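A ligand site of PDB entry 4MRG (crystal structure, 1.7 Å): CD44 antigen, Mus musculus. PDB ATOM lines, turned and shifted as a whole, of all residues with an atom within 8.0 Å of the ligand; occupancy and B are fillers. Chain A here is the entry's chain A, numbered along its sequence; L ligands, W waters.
N of Asn 6 is in hydrogen-bond range of O of Glu 18, at 2.8 Å.
The guanidinium group (NE) of Arg 59 is in salt-bridge range of the side-chain carboxylate (OE2) of Glu 18 (3.5 Å).
N of Val 7 lies within hydrogen-bond range of O of Val 130 (3.0 Å).
N of Val 130 is in hydrogen-bond range of O of Leu 5 (2.8 Å).
The side-chain amide nitrogen (ND2) of Asn 6 lies close to the backbone NH (N) of Gly 21.
The backbone NH (N) of His 16 is in hydrogen-bond range of the side-chain hydroxyl (OG1) of Thr 8, 2.9 Å away.
The side-chain amide nitrogen (ND2) of Asn 131 lies within hydrogen-bond range of the backbone carbonyl oxygen (O) of Thr 135, 3.0 Å away.
Water W2 lies within hydrogen-bond range of ND1 of His 16, O of Asn 6 and N2 of the ligand.
A nitrogen (N1) of the ligand is in salt-bridge range of the side-chain carboxylate (OE1) of Glu 18, at 2.9 Å.
The backbone carbonyl oxygen of Val 7 is in hydrogen-bond range of a nitrogen (N2) of the ligand (3.1 Å).
Asn 6 touches the ligand (CG to C6, 3.6 Å).
Thr 8 touches the ligand.
Val 130 touches the ligand (O to C8, 3.5 Å).
C of Asn 131 touches C8 of the ligand (3.7 Å).
Arg 132 touches the ligand.
Along chain A the residues within 4 Å of the ligand span positions 6 to 132.
The nearest printed residue that does not touch the ligand is His 16 (4.9 Å).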
ATOM      1  N   LEU A   5      33.433  -7.731 -15.384  1.00  0.00           N
ATOM      2  CA  LEU A   5      32.898  -8.304 -14.138  1.00  0.00           C
ATOM      3  C   LEU A   5      31.448  -8.605 -14.418  1.00  0.00           C
ATOM      4  O   LEU A   5      30.655  -7.682 -14.565  1.00  0.00           O
ATOM      5  CB  LEU A   5      33.034  -7.340 -12.945  1.00  0.00           C
ATOM      6  CG  LEU A   5      34.477  -7.007 -12.535  1.00  0.00           C
ATOM      7  CD1 LEU A   5      34.468  -5.860 -11.511  1.00  0.00           C
ATOM      8  CD2 LEU A   5      35.237  -8.187 -11.941  1.00  0.00           C
ATOM      9  N   ASN A   6      31.100  -9.891 -14.502  1.00  0.00           N
ATOM     10  CA  ASN A   6      29.729 -10.261 -14.820  1.00  0.00           C
ATOM     11  C   ASN A   6      28.993 -10.364 -13.525  1.00  0.00           C
ATOM     12  O   ASN A   6      29.412 -11.136 -12.661  1.00  0.00           O
ATOM     13  CB  ASN A   6      29.709 -11.646 -15.478  1.00  0.00           C
ATOM     14  CG  ASN A   6      30.377 -11.667 -16.820  1.00  0.00           C
ATOM     15  OD1 ASN A   6      30.497 -10.650 -17.515  1.00  0.00           O
ATOM     16  ND2 ASN A   6      30.865 -12.846 -17.191  1.00  0.00           N
ATOM     17  N   VAL A   7      27.897  -9.646 -13.390  1.00  0.00           N
ATOM     18  CA  VAL A   7      27.198  -9.592 -12.083  1.00  0.00           C
ATOM     19  C   VAL A   7      25.736 -10.010 -12.221  1.00  0.00           C
ATOM     20  O   VAL A   7      25.063  -9.781 -13.233  1.00  0.00           O
ATOM     21  CB  VAL A   7      27.255  -8.200 -11.440  1.00  0.00           C
ATOM     22  CG1 VAL A   7      28.716  -7.737 -11.212  1.00  0.00           C
ATOM     23  CG2 VAL A   7      26.538  -7.161 -12.327  1.00  0.00           C
ATOM     24  N   THR A   8      25.254 -10.637 -11.168  1.00  0.00           N
ATOM     25  CA  THR A   8      23.859 -11.089 -11.082  1.00  0.00           C
ATOM     26  C   THR A   8      22.919 -10.137 -10.341  1.00  0.00           C
ATOM     27  O   THR A   8      23.340  -9.161  -9.742  1.00  0.00           O
ATOM     28  CB  THR A   8      23.728 -12.466 -10.381  1.00  0.00           C
ATOM     29  OG1 THR A   8      24.049 -12.347  -8.976  1.00  0.00           O
ATOM     30  CG2 THR A   8      24.624 -13.509 -11.055  1.00  0.00           C
ATOM     31  N   CYS A   9      21.637 -10.456 -10.413  1.00  0.00           N
ATOM     32  CA  CYS A   9      20.657  -9.889  -9.476  1.00  0.00           C
ATOM     33  C   CYS A   9      21.159 -10.077  -8.067  1.00  0.00           C
ATOM     34  O   CYS A   9      21.907 -11.040  -7.805  1.00  0.00           O
ATOM     35  CB  CYS A   9      19.407 -10.745  -9.550  1.00  0.00           C
ATOM     36  SG  CYS A   9      18.567 -10.728 -11.150  1.00  0.00           S
ATOM     37  N   HIS A  16      26.393 -12.762  -7.303  1.00  0.00           N
ATOM     38  CA  HIS A  16      27.512 -13.542  -7.899  1.00  0.00           C
ATOM     39  C   HIS A  16      28.312 -12.671  -8.888  1.00  0.00           C
ATOM     40  O   HIS A  16      27.703 -11.924  -9.670  1.00  0.00           O
ATOM     41  CB  HIS A  16      26.892 -14.774  -8.594  1.00  0.00           C
ATOM     42  CG  HIS A  16      27.842 -15.572  -9.428  1.00  0.00           C
ATOM     43  ND1 HIS A  16      27.630 -15.800 -10.782  1.00  0.00           N
ATOM     44  CD2 HIS A  16      29.000 -16.211  -9.110  1.00  0.00           C
ATOM     45  CE1 HIS A  16      28.615 -16.551 -11.257  1.00  0.00           C
ATOM     46  NE2 HIS A  16      29.456 -16.812 -10.259  1.00  0.00           N
ATOM     47  N   VAL A  17      29.656 -12.748  -8.858  1.00  0.00           N
ATOM     48  CA  VAL A  17      30.513 -11.994  -9.775  1.00  0.00           C
ATOM     49  C   VAL A  17      31.459 -13.000 -10.452  1.00  0.00           C
ATOM     50  O   VAL A  17      32.134 -13.784  -9.761  1.00  0.00           O
ATOM     51  CB  VAL A  17      31.379 -10.945  -9.016  1.00  0.00           C
ATOM     52  CG1 VAL A  17      32.182 -10.032 -10.026  1.00  0.00           C
ATOM     53  CG2 VAL A  17      30.510 -10.071  -8.070  1.00  0.00           C
ATOM     54  N   GLU A  18      31.530 -12.958 -11.789  1.00  0.00           N
ATOM     55  CA  GLU A  18      32.533 -13.732 -12.555  1.00  0.00           C
ATOM     56  C   GLU A  18      33.494 -12.783 -13.166  1.00  0.00           C
ATOM     57  O   GLU A  18      33.043 -11.793 -13.777  1.00  0.00           O
ATOM     58  CB  GLU A  18      31.926 -14.518 -13.745  1.00  0.00           C
ATOM     59  CG  GLU A  18      30.888 -15.526 -13.407  1.00  0.00           C
ATOM     60  CD  GLU A  18      30.157 -16.040 -14.633  1.00  0.00           C
ATOM     61  OE1 GLU A  18      30.193 -15.391 -15.726  1.00  0.00           O
ATOM     62  OE2 GLU A  18      29.482 -17.065 -14.461  1.00  0.00           O
ATOM     63  N   ASN A  20      35.740 -12.021 -16.103  1.00  0.00           N
ATOM     64  CA  ASN A  20      35.933 -12.459 -17.490  1.00  0.00           C
ATOM     65  C   ASN A  20      35.189 -13.755 -17.828  1.00  0.00           C
ATOM     66  O   ASN A  20      35.542 -14.465 -18.758  1.00  0.00           O
ATOM     67  CB  ASN A  20      37.452 -12.562 -17.796  1.00  0.00           C
ATOM     68  CG  ASN A  20      38.150 -11.204 -17.720  1.00  0.00           C
ATOM     69  OD1 ASN A  20      37.584 -10.184 -18.147  1.00  0.00           O
ATOM     70  ND2 ASN A  20      39.385 -11.185 -17.193  1.00  0.00           N
ATOM     71  N   GLY A  21      34.135 -14.044 -17.075  1.00  0.00           N
ATOM     72  CA  GLY A  21      33.324 -15.186 -17.387  1.00  0.00           C
ATOM     73  C   GLY A  21      34.050 -16.522 -17.282  1.00  0.00           C
ATOM     74  O   GLY A  21      33.654 -17.486 -17.948  1.00  0.00           O
ATOM     75  N   ARG A  22      35.098 -16.598 -16.457  1.00  0.00           N
ATOM     76  CA  ARG A  22      35.884 -17.818 -16.295  1.00  0.00           C
ATOM     77  C   ARG A  22      36.452 -17.862 -14.878  1.00  0.00           C
ATOM     78  O   ARG A  22      36.791 -16.819 -14.324  1.00  0.00           O
ATOM     79  CB  ARG A  22      37.009 -17.889 -17.342  1.00  0.00           C
ATOM     80  CG  ARG A  22      37.913 -16.664 -17.412  1.00  0.00           C
ATOM     81  CD  ARG A  22      39.057 -16.868 -18.423  1.00  0.00           C
ATOM     82  NE  ARG A  22      40.124 -15.880 -18.249  1.00  0.00           N
ATOM     83  CZ  ARG A  22      40.295 -14.829 -19.048  1.00  0.00           C
ATOM     84  NH1 ARG A  22      41.286 -13.969 -18.822  1.00  0.00           N
ATOM     85  NH2 ARG A  22      39.466 -14.632 -20.063  1.00  0.00           N
ATOM     86  N   THR A  57      22.862 -20.252  -8.617  1.00  0.00           N
ATOM     87  CA  THR A  57      23.765 -20.183  -9.783  1.00  0.00           C
ATOM     88  C   THR A  57      24.184 -21.590 -10.129  1.00  0.00           C
ATOM     89  O   THR A  57      23.851 -22.548  -9.408  1.00  0.00           O
ATOM     90  CB  THR A  57      25.019 -19.412  -9.484  1.00  0.00           C
ATOM     91  OG1 THR A  57      25.890 -20.238  -8.710  1.00  0.00           O
ATOM     92  CG2 THR A  57      24.774 -18.081  -8.724  1.00  0.00           C
ATOM     93  N   CYS A  58      24.998 -21.712 -11.193  1.00  0.00           N
ATOM     94  CA  CYS A  58      25.612 -23.000 -11.521  1.00  0.00           C
ATOM     95  C   CYS A  58      27.123 -22.818 -11.512  1.00  0.00           C
ATOM     96  O   CYS A  58      27.835 -23.376 -12.389  1.00  0.00           O
ATOM     97  CB  CYS A  58      25.159 -23.454 -12.887  1.00  0.00           C
ATOM     98  SG  CYS A  58      25.606 -25.178 -13.211  1.00  0.00           S
ATOM     99  N   ARG A  59      27.595 -22.000 -10.567  1.00  0.00           N
ATOM    100  CA  ARG A  59      29.021 -21.641 -10.463  1.00  0.00           C
ATOM    101  C   ARG A  59      29.578 -21.650  -9.029  1.00  0.00           C
ATOM    102  O   ARG A  59      28.963 -21.094  -8.086  1.00  0.00           O
ATOM    103  CB  ARG A  59      29.262 -20.243 -11.047  1.00  0.00           C
ATOM    104  CG  ARG A  59      28.910 -20.132 -12.532  1.00  0.00           C
ATOM    105  CD  ARG A  59      30.030 -20.709 -13.446  1.00  0.00           C
ATOM    106  NE  ARG A  59      31.249 -19.870 -13.438  1.00  0.00           N
ATOM    107  CZ  ARG A  59      32.356 -20.073 -14.160  1.00  0.00           C
ATOM    108  NH1 ARG A  59      33.365 -19.201 -14.054  1.00  0.00           N
ATOM    109  NH2 ARG A  59      32.396 -21.074 -15.051  1.00  0.00           N
ATOM    110  N   ASP A  97      34.826 -18.191  -8.979  1.00  0.00           N
ATOM    111  CA  ASP A  97      34.168 -16.886  -9.013  1.00  0.00           C
ATOM    112  C   ASP A  97      34.070 -16.409  -7.561  1.00  0.00           C
ATOM    113  O   ASP A  97      34.648 -17.004  -6.646  1.00  0.00           O
ATOM    114  CB  ASP A  97      32.738 -17.038  -9.547  1.00  0.00           C
ATOM    115  CG  ASP A  97      32.703 -17.569 -11.008  1.00  0.00           C
ATOM    116  OD1 ASP A  97      33.738 -17.470 -11.739  1.00  0.00           O
ATOM    117  OD2 ASP A  97      31.643 -18.082 -11.404  1.00  0.00           O
ATOM    118  N   ILE A 129      31.567  -3.437 -15.699  1.00  0.00           N
ATOM    119  CA  ILE A 129      30.459  -4.179 -15.106  1.00  0.00           C
ATOM    120  C   ILE A 129      29.535  -4.652 -16.201  1.00  0.00           C
ATOM    121  O   ILE A 129      29.048  -3.838 -17.006  1.00  0.00           O
ATOM    122  CB  ILE A 129      29.652  -3.301 -14.099  1.00  0.00           C
ATOM    123  CG1 ILE A 129      30.563  -2.708 -12.989  1.00  0.00           C
ATOM    124  CG2 ILE A 129      28.499  -4.122 -13.521  1.00  0.00           C
ATOM    125  CD1 ILE A 129      31.591  -3.669 -12.409  1.00  0.00           C
ATOM    126  N   VAL A 130      29.301  -5.962 -16.277  1.00  0.00           N
ATOM    127  CA  VAL A 130      28.422  -6.510 -17.332  1.00  0.00           C
ATOM    128  C   VAL A 130      27.219  -7.132 -16.655  1.00  0.00           C
ATOM    129  O   VAL A 130      27.361  -8.134 -15.941  1.00  0.00           O
ATOM    130  CB  VAL A 130      29.132  -7.557 -18.229  1.00  0.00           C
ATOM    131  CG1 VAL A 130      28.186  -8.004 -19.379  1.00  0.00           C
ATOM    132  CG2 VAL A 130      30.500  -6.998 -18.757  1.00  0.00           C
ATOM    133  N   ASN A 131      26.031  -6.569 -16.906  1.00  0.00           N
ATOM    134  CA  ASN A 131      24.805  -7.152 -16.365  1.00  0.00           C
ATOM    135  C   ASN A 131      24.273  -8.280 -17.231  1.00  0.00           C
ATOM    136  O   ASN A 131      24.674  -8.416 -18.400  1.00  0.00           O
ATOM    137  CB  ASN A 131      23.771  -6.042 -16.199  1.00  0.00           C
ATOM    138  CG  ASN A 131      24.180  -5.102 -15.105  1.00  0.00           C
ATOM    139  OD1 ASN A 131      23.938  -5.378 -13.911  1.00  0.00           O
ATOM    140  ND2 ASN A 131      24.842  -3.998 -15.484  1.00  0.00           N
ATOM    141  N   ARG A 132      23.409  -9.108 -16.668  1.00  0.00           N
ATOM    142  CA  ARG A 132      22.914 -10.246 -17.406  1.00  0.00           C
ATOM    143  C   ARG A 132      22.071  -9.821 -18.602  1.00  0.00           C
ATOM    144  O   ARG A 132      22.048 -10.515 -19.601  1.00  0.00           O
ATOM    145  CB  ARG A 132      22.217 -11.272 -16.498  1.00  0.00           C
ATOM    146  CG  ARG A 132      21.663 -12.495 -17.204  1.00  0.00           C
ATOM    147  CD  ARG A 132      22.748 -13.396 -17.781  1.00  0.00           C
ATOM    148  NE  ARG A 132      23.315 -12.879 -19.041  1.00  0.00           N
ATOM    149  CZ  ARG A 132      24.028 -13.634 -19.883  1.00  0.00           C
ATOM    150  NH1 ARG A 132      24.218 -14.916 -19.610  1.00  0.00           N
ATOM    151  NH2 ARG A 132      24.527 -13.114 -20.982  1.00  0.00           N
ATOM    152  N   ASP A 133      21.405  -8.647 -18.512  1.00  0.00           N
ATOM    153  CA  ASP A 133      20.676  -8.098 -19.682  1.00  0.00           C
ATOM    154  C   ASP A 133      21.531  -7.332 -20.680  1.00  0.00           C
ATOM    155  O   ASP A 133      21.007  -6.779 -21.657  1.00  0.00           O
ATOM    156  CB  ASP A 133      19.490  -7.239 -19.231  1.00  0.00           C
ATOM    157  CG  ASP A 133      19.914  -5.914 -18.579  1.00  0.00           C
ATOM    158  OD1 ASP A 133      21.142  -5.640 -18.524  1.00  0.00           O
ATOM    159  OD2 ASP A 133      18.992  -5.196 -18.092  1.00  0.00           O
ATOM    160  N   GLY A 134      22.858  -7.348 -20.462  1.00  0.00           N
ATOM    161  CA  GLY A 134      23.835  -6.803 -21.375  1.00  0.00           C
ATOM    162  C   GLY A 134      24.192  -5.376 -21.050  1.00  0.00           C
ATOM    163  O   GLY A 134      25.144  -4.864 -21.612  1.00  0.00           O
ATOM    164  N   THR A 135      23.450  -4.740 -20.139  1.00  0.00           N
ATOM    165  CA  THR A 135      23.757  -3.370 -19.759  1.00  0.00           C
ATOM    166  C   THR A 135      25.203  -3.302 -19.221  1.00  0.00           C
ATOM    167  O   THR A 135      25.594  -4.125 -18.400  1.00  0.00           O
ATOM    168  CB  THR A 135      22.774  -2.848 -18.660  1.00  0.00           C
ATOM    169  OG1 THR A 135      21.413  -3.009 -19.082  1.00  0.00           O
ATOM    170  CG2 THR A 135      23.026  -1.349 -18.455  1.00  0.00           C
ATOM    171  N   ARG A 136      25.967  -2.289 -19.642  1.00  0.00           N
ATOM    172  CA  ARG A 136      27.373  -2.155 -19.222  1.00  0.00           C
ATOM    173  C   ARG A 136      27.685  -0.786 -18.650  1.00  0.00           C
ATOM    174  O   ARG A 136      27.103   0.234 -19.069  1.00  0.00           O
ATOM    175  CB  ARG A 136      28.354  -2.465 -20.357  1.00  0.00           C
ATOM    176  CG  ARG A 136      28.671  -3.962 -20.534  1.00  0.00           C
ATOM    177  CD  ARG A 136      29.607  -4.206 -21.759  1.00  0.00           C
ATOM    178  NE  ARG A 136      29.553  -5.599 -22.189  1.00  0.00           N
ATOM    179  CZ  ARG A 136      30.599  -6.404 -22.360  1.00  0.00           C
ATOM    180  NH1 ARG A 136      31.881  -5.976 -22.170  1.00  0.00           N
ATOM    181  NH2 ARG A 136      30.357  -7.654 -22.763  1.00  0.00           N
HETATM  182  C1  LIG L   1      27.687 -15.085 -18.080  1.00  0.00           C
HETATM  183  N1  LIG L   1      27.826 -16.200 -17.100  1.00  0.00           N
HETATM  184  C2  LIG L   1      26.629 -16.271 -16.253  1.00  0.00           C
HETATM  185  C3  LIG L   1      26.477 -14.993 -15.437  1.00  0.00           C
HETATM  186  C4  LIG L   1      26.555 -13.811 -16.264  1.00  0.00           C
HETATM  187  C5  LIG L   1      27.170 -13.859 -17.533  1.00  0.00           C
HETATM  188  C6  LIG L   1      27.233 -12.661 -18.271  1.00  0.00           C
HETATM  189  C7  LIG L   1      26.725 -11.451 -17.772  1.00  0.00           C
HETATM  190  C8  LIG L   1      26.142 -11.394 -16.478  1.00  0.00           C
HETATM  191  C9  LIG L   1      26.074 -12.585 -15.761  1.00  0.00           C
HETATM  192  N2  LIG L   1      25.498 -12.586 -14.505  1.00  0.00           N
HETATM  193  O   HOH W   1      22.949 -13.813 -14.216  1.00  0.00           O
HETATM  194  O   HOH W   2      27.709 -13.521 -12.607  1.00  0.00           O
